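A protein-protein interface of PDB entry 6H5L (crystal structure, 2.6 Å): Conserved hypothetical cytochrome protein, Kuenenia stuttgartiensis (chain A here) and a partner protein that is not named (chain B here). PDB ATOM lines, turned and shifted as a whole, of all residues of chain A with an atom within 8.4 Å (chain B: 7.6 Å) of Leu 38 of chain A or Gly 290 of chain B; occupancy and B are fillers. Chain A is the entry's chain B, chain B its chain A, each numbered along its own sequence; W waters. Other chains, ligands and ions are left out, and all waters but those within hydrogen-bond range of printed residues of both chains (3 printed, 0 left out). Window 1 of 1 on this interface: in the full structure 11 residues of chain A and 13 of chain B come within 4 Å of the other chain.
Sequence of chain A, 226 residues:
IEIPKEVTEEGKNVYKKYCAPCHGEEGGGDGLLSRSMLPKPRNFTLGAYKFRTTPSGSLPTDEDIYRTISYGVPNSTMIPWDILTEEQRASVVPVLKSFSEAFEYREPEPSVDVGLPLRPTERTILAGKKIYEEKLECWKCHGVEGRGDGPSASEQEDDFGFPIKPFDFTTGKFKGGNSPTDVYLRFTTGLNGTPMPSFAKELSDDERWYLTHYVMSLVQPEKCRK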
ATOM      1  N   LEU A  33       3.123 -11.993 -13.960  1.00  0.00           N
ATOM      2  CA  LEU A  33       4.334 -12.426 -14.647  1.00  0.00           C
ATOM      3  C   LEU A  33       5.554 -11.588 -14.291  1.00  0.00           C
ATOM      4  O   LEU A  33       6.660 -11.937 -14.713  1.00  0.00           O
ATOM      5  CB  LEU A  33       4.113 -12.405 -16.161  1.00  0.00           C
ATOM      6  CG  LEU A  33       3.611 -13.686 -16.838  1.00  0.00           C
ATOM      7  CD1 LEU A  33       2.790 -14.543 -15.886  1.00  0.00           C
ATOM      8  CD2 LEU A  33       2.790 -13.341 -18.072  1.00  0.00           C
ATOM      9  N   SER A  34       5.385 -10.501 -13.535  1.00  0.00           N
ATOM     10  CA  SER A  34       6.531  -9.703 -13.117  1.00  0.00           C
ATOM     11  C   SER A  34       7.366 -10.402 -12.051  1.00  0.00           C
ATOM     12  O   SER A  34       8.529 -10.034 -11.855  1.00  0.00           O
ATOM     13  CB  SER A  34       6.064  -8.344 -12.595  1.00  0.00           C
ATOM     14  OG  SER A  34       5.303  -8.485 -11.409  1.00  0.00           O
ATOM     15  N   ARG A  35       6.800 -11.396 -11.362  1.00  0.00           N
ATOM     16  CA  ARG A  35       7.539 -12.093 -10.313  1.00  0.00           C
ATOM     17  C   ARG A  35       8.732 -12.860 -10.872  1.00  0.00           C
ATOM     18  O   ARG A  35       9.748 -13.005 -10.185  1.00  0.00           O
ATOM     19  CB  ARG A  35       6.610 -13.047  -9.563  1.00  0.00           C
ATOM     20  CG  ARG A  35       6.105 -14.194 -10.423  1.00  0.00           C
ATOM     21  CD  ARG A  35       5.110 -15.080  -9.701  1.00  0.00           C
ATOM     22  NE  ARG A  35       4.574 -16.099 -10.598  1.00  0.00           N
ATOM     23  CZ  ARG A  35       3.729 -17.054 -10.231  1.00  0.00           C
ATOM     24  NH1 ARG A  35       3.316 -17.128  -8.973  1.00  0.00           N
ATOM     25  NH2 ARG A  35       3.296 -17.937 -11.120  1.00  0.00           N
ATOM     26  N   SER A  36       8.632 -13.348 -12.107  1.00  0.00           N
ATOM     27  CA  SER A  36       9.668 -14.171 -12.718  1.00  0.00           C
ATOM     28  C   SER A  36      10.363 -13.469 -13.874  1.00  0.00           C
ATOM     29  O   SER A  36      11.132 -14.104 -14.602  1.00  0.00           O
ATOM     30  CB  SER A  36       9.072 -15.494 -13.199  1.00  0.00           C
ATOM     31  OG  SER A  36       8.110 -15.276 -14.217  1.00  0.00           O
ATOM     32  N   MET A  37      10.114 -12.178 -14.060  1.00  0.00           N
ATOM     33  CA  MET A  37      10.596 -11.443 -15.217  1.00  0.00           C
ATOM     34  C   MET A  37      11.812 -10.607 -14.846  1.00  0.00           C
ATOM     35  O   MET A  37      11.841  -9.974 -13.788  1.00  0.00           O
ATOM     36  CB  MET A  37       9.489 -10.548 -15.775  1.00  0.00           C
ATOM     37  CG  MET A  37       9.813  -9.885 -17.096  1.00  0.00           C
ATOM     38  SD  MET A  37       8.357  -9.107 -17.822  1.00  0.00           S
ATOM     39  CE  MET A  37       7.329 -10.540 -18.133  1.00  0.00           C
ATOM     40  N   LEU A  38      12.813 -10.610 -15.722  1.00  0.00           N
ATOM     41  CA  LEU A  38      14.028  -9.826 -15.532  1.00  0.00           C
ATOM     42  C   LEU A  38      14.519  -9.321 -16.884  1.00  0.00           C
ATOM     43  O   LEU A  38      14.837 -10.131 -17.764  1.00  0.00           O
ATOM     44  CB  LEU A  38      15.110 -10.657 -14.841  1.00  0.00           C
ATOM     45  CG  LEU A  38      14.918 -10.936 -13.349  1.00  0.00           C
ATOM     46  CD1 LEU A  38      15.767 -12.115 -12.905  1.00  0.00           C
ATOM     47  CD2 LEU A  38      15.258  -9.698 -12.539  1.00  0.00           C
ATOM     48  N   PRO A  39      14.604  -7.995 -17.099  1.00  0.00           N
ATOM     49  CA  PRO A  39      14.317  -6.890 -16.171  1.00  0.00           C
ATOM     50  C   PRO A  39      12.848  -6.784 -15.761  1.00  0.00           C
ATOM     51  O   PRO A  39      11.966  -7.214 -16.504  1.00  0.00           O
ATOM     52  CB  PRO A  39      14.732  -5.645 -16.966  1.00  0.00           C
ATOM     53  CG  PRO A  39      15.638  -6.147 -18.036  1.00  0.00           C
ATOM     54  CD  PRO A  39      15.108  -7.497 -18.388  1.00  0.00           C
ATOM     55  N   LYS A  40      12.608  -6.221 -14.582  1.00  0.00           N
ATOM     56  CA  LYS A  40      11.251  -6.060 -14.091  1.00  0.00           C
ATOM     57  C   LYS A  40      10.490  -5.051 -14.951  1.00  0.00           C
ATOM     58  O   LYS A  40      11.075  -4.083 -15.443  1.00  0.00           O
ATOM     59  CB  LYS A  40      11.265  -5.592 -12.637  1.00  0.00           C
ATOM     60  CG  LYS A  40      11.834  -6.605 -11.663  1.00  0.00           C
ATOM     61  CD  LYS A  40      10.972  -7.854 -11.608  1.00  0.00           C
ATOM     62  CE  LYS A  40      11.614  -8.934 -10.754  1.00  0.00           C
ATOM     63  NZ  LYS A  40      10.846 -10.210 -10.809  1.00  0.00           N
ATOM     64  N   PRO A  41       9.186  -5.258 -15.152  1.00  0.00           N
ATOM     65  CA  PRO A  41       8.403  -4.280 -15.915  1.00  0.00           C
ATOM     66  C   PRO A  41       8.269  -2.977 -15.143  1.00  0.00           C
ATOM     67  O   PRO A  41       8.189  -2.968 -13.912  1.00  0.00           O
ATOM     68  CB  PRO A  41       7.052  -4.975 -16.103  1.00  0.00           C
ATOM     69  CG  PRO A  41       6.959  -5.906 -14.957  1.00  0.00           C
ATOM     70  CD  PRO A  41       8.362  -6.387 -14.700  1.00  0.00           C
ATOM     71  N   ASN A  75      16.632  -5.838 -24.969  1.00  0.00           N
ATOM     72  CA  ASN A  75      17.169  -6.488 -23.771  1.00  0.00           C
ATOM     73  C   ASN A  75      16.114  -6.598 -22.674  1.00  0.00           C
ATOM     74  O   ASN A  75      16.429  -6.518 -21.483  1.00  0.00           O
ATOM     75  CB  ASN A  75      18.414  -5.765 -23.248  1.00  0.00           C
ATOM     76  CG  ASN A  75      19.495  -5.628 -24.303  1.00  0.00           C
ATOM     77  OD1 ASN A  75      19.893  -6.607 -24.935  1.00  0.00           O
ATOM     78  ND2 ASN A  75      19.967  -4.404 -24.508  1.00  0.00           N
ATOM     79  N   SER A  76      14.857  -6.780 -23.072  1.00  0.00           N
ATOM     80  CA  SER A  76      13.749  -6.937 -22.139  1.00  0.00           C
ATOM     81  C   SER A  76      12.563  -7.504 -22.904  1.00  0.00           C
ATOM     82  O   SER A  76      12.575  -7.589 -24.135  1.00  0.00           O
ATOM     83  CB  SER A  76      13.379  -5.613 -21.467  1.00  0.00           C
ATOM     84  OG  SER A  76      12.688  -4.763 -22.367  1.00  0.00           O
ATOM     85  N   THR A  77      11.530  -7.884 -22.156  1.00  0.00           N
ATOM     86  CA  THR A  77      10.305  -8.405 -22.750  1.00  0.00           C
ATOM     87  C   THR A  77       9.415  -7.312 -23.326  1.00  0.00           C
ATOM     88  O   THR A  77       8.306  -7.616 -23.782  1.00  0.00           O
ATOM     89  CB  THR A  77       9.522  -9.210 -21.708  1.00  0.00           C
ATOM     90  OG1 THR A  77       9.195  -8.366 -20.601  1.00  0.00           O
ATOM     91  CG2 THR A  77      10.351 -10.384 -21.214  1.00  0.00           C
ATOM     92  N   SER A 154      27.795  -5.623 -10.279  1.00  0.00           N
ATOM     93  CA  SER A 154      26.822  -6.518  -9.661  1.00  0.00           C
ATOM     94  C   SER A 154      26.025  -5.855  -8.544  1.00  0.00           C
ATOM     95  O   SER A 154      24.941  -6.340  -8.203  1.00  0.00           O
ATOM     96  CB  SER A 154      27.525  -7.765  -9.121  1.00  0.00           C
ATOM     97  OG  SER A 154      28.071  -8.542 -10.174  1.00  0.00           O
ATOM     98  N   ASP A 158      18.089  -0.414  -8.636  1.00  0.00           N
ATOM     99  CA  ASP A 158      17.082   0.558  -9.034  1.00  0.00           C
ATOM    100  C   ASP A 158      16.773   1.518  -7.887  1.00  0.00           C
ATOM    101  O   ASP A 158      17.201   1.337  -6.745  1.00  0.00           O
ATOM    102  CB  ASP A 158      15.787  -0.144  -9.448  1.00  0.00           C
ATOM    103  CG  ASP A 158      15.841  -0.705 -10.849  1.00  0.00           C
ATOM    104  OD1 ASP A 158      16.591  -0.163 -11.687  1.00  0.00           O
ATOM    105  OD2 ASP A 158      15.119  -1.688 -11.114  1.00  0.00           O
ATOM    106  N   PHE A 162      15.472  -2.790  -6.996  1.00  0.00           N
ATOM    107  CA  PHE A 162      15.816  -3.986  -7.749  1.00  0.00           C
ATOM    108  C   PHE A 162      17.235  -3.903  -8.293  1.00  0.00           C
ATOM    109  O   PHE A 162      17.695  -2.820  -8.671  1.00  0.00           O
ATOM    110  CB  PHE A 162      14.850  -4.194  -8.916  1.00  0.00           C
ATOM    111  CG  PHE A 162      13.516  -4.739  -8.507  1.00  0.00           C
ATOM    112  CD1 PHE A 162      13.345  -6.099  -8.297  1.00  0.00           C
ATOM    113  CD2 PHE A 162      12.429  -3.899  -8.342  1.00  0.00           C
ATOM    114  CE1 PHE A 162      12.117  -6.608  -7.923  1.00  0.00           C
ATOM    115  CE2 PHE A 162      11.197  -4.400  -7.970  1.00  0.00           C
ATOM    116  CZ  PHE A 162      11.041  -5.757  -7.760  1.00  0.00           C
ATOM    117  N   PRO A 163      17.928  -5.038  -8.328  1.00  0.00           N
ATOM    118  CA  PRO A 163      19.229  -5.091  -9.003  1.00  0.00           C
ATOM    119  C   PRO A 163      19.112  -4.645 -10.452  1.00  0.00           C
ATOM    120  O   PRO A 163      18.260  -5.129 -11.204  1.00  0.00           O
ATOM    121  CB  PRO A 163      19.618  -6.570  -8.901  1.00  0.00           C
ATOM    122  CG  PRO A 163      18.835  -7.100  -7.739  1.00  0.00           C
ATOM    123  CD  PRO A 163      17.562  -6.318  -7.698  1.00  0.00           C
ATOM    124  N   ILE A 164      19.961  -3.694 -10.841  1.00  0.00           N
ATOM    125  CA  ILE A 164      20.096  -3.280 -12.237  1.00  0.00           C
ATOM    126  C   ILE A 164      21.584  -3.371 -12.572  1.00  0.00           C
ATOM    127  O   ILE A 164      22.336  -2.399 -12.454  1.00  0.00           O
ATOM    128  CB  ILE A 164      19.524  -1.879 -12.503  1.00  0.00           C
ATOM    129  CG1 ILE A 164      19.722  -1.459 -13.963  1.00  0.00           C
ATOM    130  CG2 ILE A 164      20.072  -0.838 -11.524  1.00  0.00           C
ATOM    131  CD1 ILE A 164      18.812  -0.323 -14.392  1.00  0.00           C
ATOM    132  N   LYS A 165      22.014  -4.545 -13.006  1.00  0.00           N
ATOM    133  CA  LYS A 165      23.386  -4.746 -13.449  1.00  0.00           C
ATOM    134  C   LYS A 165      23.489  -4.326 -14.907  1.00  0.00           C
ATOM    135  O   LYS A 165      22.752  -4.865 -15.743  1.00  0.00           O
ATOM    136  CB  LYS A 165      23.787  -6.199 -13.284  1.00  0.00           C
ATOM    137  CG  LYS A 165      25.215  -6.516 -13.667  1.00  0.00           C
ATOM    138  CD  LYS A 165      25.569  -7.947 -13.285  1.00  0.00           C
ATOM    139  CE  LYS A 165      26.955  -8.345 -13.783  1.00  0.00           C
ATOM    140  NZ  LYS A 165      27.056  -8.426 -15.271  1.00  0.00           N
ATOM    141  N   LYS A 175      18.831   0.033 -24.963  1.00  0.00           N
ATOM    142  CA  LYS A 175      17.428   0.001 -24.565  1.00  0.00           C
ATOM    143  C   LYS A 175      16.659   1.192 -25.123  1.00  0.00           C
ATOM    144  O   LYS A 175      15.486   1.060 -25.496  1.00  0.00           O
ATOM    145  CB  LYS A 175      17.319  -0.049 -23.042  1.00  0.00           C
ATOM    146  CG  LYS A 175      17.799  -1.355 -22.432  1.00  0.00           C
ATOM    147  CD  LYS A 175      17.287  -1.525 -21.013  1.00  0.00           C
ATOM    148  CE  LYS A 175      17.712  -2.865 -20.436  1.00  0.00           C
ATOM    149  NZ  LYS A 175      17.069  -3.118 -19.118  1.00  0.00           N
ATOM    150  N   LEU B 266      28.870 -17.268 -12.589  1.00  0.00           N
ATOM    151  CA  LEU B 266      27.452 -17.587 -12.736  1.00  0.00           C
ATOM    152  C   LEU B 266      26.652 -16.388 -13.228  1.00  0.00           C
ATOM    153  O   LEU B 266      25.720 -16.542 -14.027  1.00  0.00           O
ATOM    154  CB  LEU B 266      26.894 -18.101 -11.409  1.00  0.00           C
ATOM    155  CG  LEU B 266      27.457 -19.442 -10.942  1.00  0.00           C
ATOM    156  CD1 LEU B 266      27.094 -19.701  -9.490  1.00  0.00           C
ATOM    157  CD2 LEU B 266      26.949 -20.564 -11.833  1.00  0.00           C
ATOM    158  N   VAL B 267      27.003 -15.183 -12.771  1.00  0.00           N
ATOM    159  CA  VAL B 267      26.254 -13.998 -13.170  1.00  0.00           C
ATOM    160  C   VAL B 267      26.465 -13.662 -14.643  1.00  0.00           C
ATOM    161  O   VAL B 267      25.643 -12.956 -15.238  1.00  0.00           O
ATOM    162  CB  VAL B 267      26.626 -12.803 -12.269  1.00  0.00           C
ATOM    163  CG1 VAL B 267      27.971 -12.212 -12.676  1.00  0.00           C
ATOM    164  CG2 VAL B 267      25.530 -11.745 -12.293  1.00  0.00           C
ATOM    165  N   TYR B 286      21.930 -18.933  -7.152  1.00  0.00           N
ATOM    166  CA  TYR B 286      21.106 -17.767  -7.435  1.00  0.00           C
ATOM    167  C   TYR B 286      20.434 -17.282  -6.157  1.00  0.00           C
ATOM    168  O   TYR B 286      19.797 -18.065  -5.441  1.00  0.00           O
ATOM    169  CB  TYR B 286      20.059 -18.122  -8.495  1.00  0.00           C
ATOM    170  CG  TYR B 286      19.146 -16.985  -8.899  1.00  0.00           C
ATOM    171  CD1 TYR B 286      19.469 -16.152  -9.961  1.00  0.00           C
ATOM    172  CD2 TYR B 286      17.945 -16.763  -8.235  1.00  0.00           C
ATOM    173  CE1 TYR B 286      18.630 -15.123 -10.343  1.00  0.00           C
ATOM    174  CE2 TYR B 286      17.100 -15.738  -8.612  1.00  0.00           C
ATOM    175  CZ  TYR B 286      17.449 -14.920  -9.666  1.00  0.00           C
ATOM    176  OH  TYR B 286      16.619 -13.892 -10.052  1.00  0.00           O
ATOM    177  N   GLU B 287      20.587 -15.986  -5.867  1.00  0.00           N
ATOM    178  CA  GLU B 287      19.989 -15.384  -4.680  1.00  0.00           C
ATOM    179  C   GLU B 287      18.611 -14.797  -4.964  1.00  0.00           C
ATOM    180  O   GLU B 287      17.611 -15.321  -4.463  1.00  0.00           O
ATOM    181  CB  GLU B 287      20.917 -14.306  -4.114  1.00  0.00           C
ATOM    182  CG  GLU B 287      20.371 -13.626  -2.871  1.00  0.00           C
ATOM    183  CD  GLU B 287      21.378 -12.708  -2.222  1.00  0.00           C
ATOM    184  OE1 GLU B 287      21.101 -12.224  -1.106  1.00  0.00           O
ATOM    185  OE2 GLU B 287      22.446 -12.478  -2.824  1.00  0.00           O
ATOM    186  N   LYS B 288      18.536 -13.744  -5.792  1.00  0.00           N
ATOM    187  CA  LYS B 288      17.266 -13.147  -6.205  1.00  0.00           C
ATOM    188  C   LYS B 288      17.463 -12.068  -7.265  1.00  0.00           C
ATOM    189  O   LYS B 288      18.477 -11.363  -7.254  1.00  0.00           O
ATOM    190  CB  LYS B 288      16.522 -12.547  -5.007  1.00  0.00           C
ATOM    191  CG  LYS B 288      17.318 -11.517  -4.220  1.00  0.00           C
ATOM    192  CD  LYS B 288      16.497 -10.931  -3.085  1.00  0.00           C
ATOM    193  CE  LYS B 288      17.342 -10.036  -2.197  1.00  0.00           C
ATOM    194  NZ  LYS B 288      16.530  -9.491  -1.075  1.00  0.00           N
ATOM    195  N   HIS B 289      16.493 -11.919  -8.171  1.00  0.00           N
ATOM    196  CA  HIS B 289      16.432 -10.766  -9.077  1.00  0.00           C
ATOM    197  C   HIS B 289      17.725 -10.598  -9.879  1.00  0.00           C
ATOM    198  O   HIS B 289      18.256  -9.496 -10.024  1.00  0.00           O
ATOM    199  CB  HIS B 289      16.100  -9.490  -8.297  1.00  0.00           C
ATOM    200  CG  HIS B 289      14.866  -9.607  -7.457  1.00  0.00           C
ATOM    201  ND1 HIS B 289      13.736 -10.263  -7.892  1.00  0.00           N
ATOM    202  CD2 HIS B 289      14.587  -9.164  -6.209  1.00  0.00           C
ATOM    203  CE1 HIS B 289      12.810 -10.215  -6.951  1.00  0.00           C
ATOM    204  NE2 HIS B 289      13.301  -9.554  -5.919  1.00  0.00           N
ATOM    205  N   GLY B 290      18.239 -11.712 -10.398  1.00  0.00           N
ATOM    206  CA  GLY B 290      19.443 -11.694 -11.210  1.00  0.00           C
ATOM    207  C   GLY B 290      20.742 -11.584 -10.440  1.00  0.00           C
ATOM    208  O   GLY B 290      21.797 -11.392 -11.057  1.00  0.00           O
ATOM    209  N   ARG B 291      20.696 -11.700  -9.115  1.00  0.00           N
ATOM    210  CA  ARG B 291      21.861 -11.575  -8.251  1.00  0.00           C
ATOM    211  C   ARG B 291      22.260 -12.957  -7.755  1.00  0.00           C
ATOM    212  O   ARG B 291      21.412 -13.716  -7.277  1.00  0.00           O
ATOM    213  CB  ARG B 291      21.543 -10.659  -7.068  1.00  0.00           C
ATOM    214  CG  ARG B 291      22.703  -9.863  -6.489  1.00  0.00           C
ATOM    215  CD  ARG B 291      22.202  -9.101  -5.266  1.00  0.00           C
ATOM    216  NE  ARG B 291      22.898  -7.842  -5.012  1.00  0.00           N
ATOM    217  CZ  ARG B 291      22.712  -6.729  -5.714  1.00  0.00           C
ATOM    218  NH1 ARG B 291      21.873  -6.721  -6.737  1.00  0.00           N
ATOM    219  NH2 ARG B 291      23.374  -5.626  -5.400  1.00  0.00           N
ATOM    220  N   PHE B 292      23.541 -13.282  -7.869  1.00  0.00           N
ATOM    221  CA  PHE B 292      24.062 -14.548  -7.379  1.00  0.00           C
ATOM    222  C   PHE B 292      24.854 -14.333  -6.094  1.00  0.00           C
ATOM    223  O   PHE B 292      25.246 -13.212  -5.758  1.00  0.00           O
ATOM    224  CB  PHE B 292      24.937 -15.223  -8.439  1.00  0.00           C
ATOM    225  CG  PHE B 292      24.158 -15.835  -9.572  1.00  0.00           C
ATOM    226  CD1 PHE B 292      23.746 -15.064 -10.646  1.00  0.00           C
ATOM    227  CD2 PHE B 292      23.843 -17.185  -9.566  1.00  0.00           C
ATOM    228  CE1 PHE B 292      23.031 -15.627 -11.688  1.00  0.00           C
ATOM    229  CE2 PHE B 292      23.129 -17.752 -10.604  1.00  0.00           C
ATOM    230  CZ  PHE B 292      22.724 -16.973 -11.666  1.00  0.00           C
ATOM    231  N   TYR B 345      11.724 -16.259  -6.380  1.00  0.00           N
ATOM    232  CA  TYR B 345      13.122 -16.273  -6.798  1.00  0.00           C
ATOM    233  C   TYR B 345      13.445 -17.542  -7.575  1.00  0.00           C
ATOM    234  O   TYR B 345      14.187 -17.500  -8.563  1.00  0.00           O
ATOM    235  CB  TYR B 345      14.044 -16.143  -5.584  1.00  0.00           C
ATOM    236  CG  TYR B 345      13.765 -14.950  -4.693  1.00  0.00           C
ATOM    237  CD1 TYR B 345      13.160 -13.803  -5.193  1.00  0.00           C
ATOM    238  CD2 TYR B 345      14.111 -14.975  -3.348  1.00  0.00           C
ATOM    239  CE1 TYR B 345      12.905 -12.718  -4.375  1.00  0.00           C
ATOM    240  CE2 TYR B 345      13.861 -13.895  -2.525  1.00  0.00           C
ATOM    241  CZ  TYR B 345      13.258 -12.769  -3.043  1.00  0.00           C
ATOM    242  OH  TYR B 345      13.008 -11.691  -2.226  1.00  0.00           O
ATOM    243  N   LEU B 347      11.267 -19.143  -9.390  1.00  0.00           N
ATOM    244  CA  LEU B 347      10.603 -18.987 -10.679  1.00  0.00           C
ATOM    245  C   LEU B 347      11.401 -18.092 -11.617  1.00  0.00           C
ATOM    246  O   LEU B 347      11.308 -18.240 -12.841  1.00  0.00           O
ATOM    247  CB  LEU B 347       9.191 -18.437 -10.476  1.00  0.00           C
ATOM    248  CG  LEU B 347       8.219 -19.406  -9.799  1.00  0.00           C
ATOM    249  CD1 LEU B 347       6.859 -18.760  -9.575  1.00  0.00           C
ATOM    250  CD2 LEU B 347       8.082 -20.679 -10.621  1.00  0.00           C
ATOM    251  N   GLU B 348      12.193 -17.165 -11.071  1.00  0.00           N
ATOM    252  CA  GLU B 348      13.072 -16.362 -11.915  1.00  0.00           C
ATOM    253  C   GLU B 348      14.139 -17.226 -12.575  1.00  0.00           C
ATOM    254  O   GLU B 348      14.531 -16.973 -13.720  1.00  0.00           O
ATOM    255  CB  GLU B 348      13.716 -15.244 -11.097  1.00  0.00           C
ATOM    256  CG  GLU B 348      12.725 -14.288 -10.457  1.00  0.00           C
ATOM    257  CD  GLU B 348      13.400 -13.088  -9.826  1.00  0.00           C
ATOM    258  OE1 GLU B 348      13.039 -11.946 -10.180  1.00  0.00           O
ATOM    259  OE2 GLU B 348      14.299 -13.287  -8.984  1.00  0.00           O
ATOM    260  N   VAL B 349      14.617 -18.253 -11.870  1.00  0.00           N
ATOM    261  CA  VAL B 349      15.581 -19.175 -12.461  1.00  0.00           C
ATOM    262  C   VAL B 349      14.921 -20.000 -13.558  1.00  0.00           C
ATOM    263  O   VAL B 349      15.421 -20.077 -14.686  1.00  0.00           O
ATOM    264  CB  VAL B 349      16.200 -20.076 -11.378  1.00  0.00           C
ATOM    265  CG1 VAL B 349      16.945 -21.241 -12.014  1.00  0.00           C
ATOM    266  CG2 VAL B 349      17.131 -19.276 -10.494  1.00  0.00           C
ATOM    267  N   ALA B 351      12.209 -19.480 -15.240  1.00  0.00           N
ATOM    268  CA  ALA B 351      11.651 -18.713 -16.348  1.00  0.00           C
ATOM    269  C   ALA B 351      12.677 -18.426 -17.435  1.00  0.00           C
ATOM    270  O   ALA B 351      12.293 -18.049 -18.548  1.00  0.00           O
ATOM    271  CB  ALA B 351      11.053 -17.400 -15.844  1.00  0.00           C
ATOM    272  N   LYS B 352      13.968 -18.589 -17.143  1.00  0.00           N
ATOM    273  CA  LYS B 352      14.994 -18.369 -18.155  1.00  0.00           C
ATOM    274  C   LYS B 352      14.968 -19.431 -19.247  1.00  0.00           C
ATOM    275  O   LYS B 352      15.491 -19.190 -20.339  1.00  0.00           O
ATOM    276  CB  LYS B 352      16.373 -18.324 -17.496  1.00  0.00           C
ATOM    277  CG  LYS B 352      16.542 -17.189 -16.496  1.00  0.00           C
ATOM    278  CD  LYS B 352      17.856 -17.297 -15.741  1.00  0.00           C
ATOM    279  CE  LYS B 352      18.071 -16.093 -14.845  1.00  0.00           C
ATOM    280  NZ  LYS B 352      18.108 -14.837 -15.642  1.00  0.00           N
HETATM  281  O   HOH W   1      13.451 -15.000 -15.645  1.00  0.00           O
HETATM  282  O   HOH W   2      25.317 -10.434 -16.125  1.00  0.00           O
HETATM  283  O   HOH W   3      15.967 -13.419 -17.669  1.00  0.00           O
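Printed residues of chain B within 4 Å of Ser 36 of chain A: Leu 347, Glu 348 and Ala 351.
Met 37 of chain A touches none of the printed residues of chain B.
Of the printed residues of chain B, Ser 154 of chain A touches Arg 291.
Printed residues of chain A within 4 Å of Tyr 286 of chain B: Leu 38.
Of chain A, only Leu 38 (3.5 Å) comes within 4 Å of Gly 290 of chain B.
The nearest residue of chain B that does not touch Leu 38 of chain A is Lys 352 of chain B (4.5 Å).
Printed residues of chain A that touch a printed residue of chain B: Arg 35, Ser 36, Leu 38, Lys 40, Ser 154, Phe 162, Pro 163 and Lys 165.
Hydrophobic or aromatic side chains of chain A within 4 Å of the printed part of chain B: Leu 38, Phe 162 and Pro 163.
Hydrophobic or aromatic side chains of chain B within 4 Å of the printed part of chain A: Val 267, Tyr 286, His 289, Leu 347 and Ala 351.
O of Arg 35 of chain A lies within hydrogen-bond range of NZ of Lys 40 of chain A (3.1 Å).
The side-chain hydroxyl of Tyr 286 of chain B sits at hydrogen-bond distance from the backbone NH of Gly 290 of chain B, 2.7 Å away.
The side-chain hydroxyl (OH) of Tyr 286 of chain B lies within hydrogen-bond range of the side-chain carboxylate (OE2) of Glu 348 of chain B (2.6 Å).
The backbone carbonyl oxygen (O) of Ser 34 of chain A is in hydrogen-bond range of the side-chain amino group (NZ) of Lys 40 of chain A, at 2.5 Å.
O of Met 37 of chain A lies within hydrogen-bond range of NZ of Lys 40 of chain A (3.1 Å).
N of His 289 of chain B sits at hydrogen-bond distance from OE2 of Glu 348 of chain B, at 2.7 Å.
Arg 35 of chain A touches Leu 347 of chain B (CZ to CD1, 3.6 Å).
CB of Ser 36 of chain A touches O of Leu 347 of chain B (3.6 Å).
Ser 36 of chain A touches Glu 348 of chain B.
O of Ser 36 of chain A touches CB of Ala 351 of chain B, at 3.5 Å.
His 289 of chain B touches Leu 38 of chain A.
Leu 38 of chain A touches Glu 348 of chain B.
Phe 162 of chain A touches His 289 of chain B.
Pro 163 of chain A touches His 289 of chain B (CG to O, 3.4 Å).
Pro 163 of chain A touches Arg 291 of chain B.
Lys 165 of chain A touches Val 267 of chain B (CD to CG2, 3.9 Å).
Water W2 bridges O of Val 267 of chain B and NZ of Lys 165 of chain A.
Water W1 lies within hydrogen-bond range of the backbone carbonyl oxygen of Ser 36 of chain A and the backbone carbonyl oxygen of Glu 348 of chain B.
Water W3 bridges NZ of Lys 352 of chain B (3.3 Å) and O of Leu 38 of chain A (3.5 Å).
The backbone carbonyl oxygen (O) of Ser 154 of chain A lies within hydrogen-bond range of the guanidinium group (NH2) of Arg 291 of chain B.
The backbone carbonyl oxygen of Arg 35 of chain A lies close to the side-chain carboxylate of Glu 348 of chain B (3.5 Å).
The side-chain carboxylate (OE1) of Glu 348 of chain B is in salt-bridge range of the side-chain amino group (NZ) of Lys 40 of chain A (2.9 Å).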
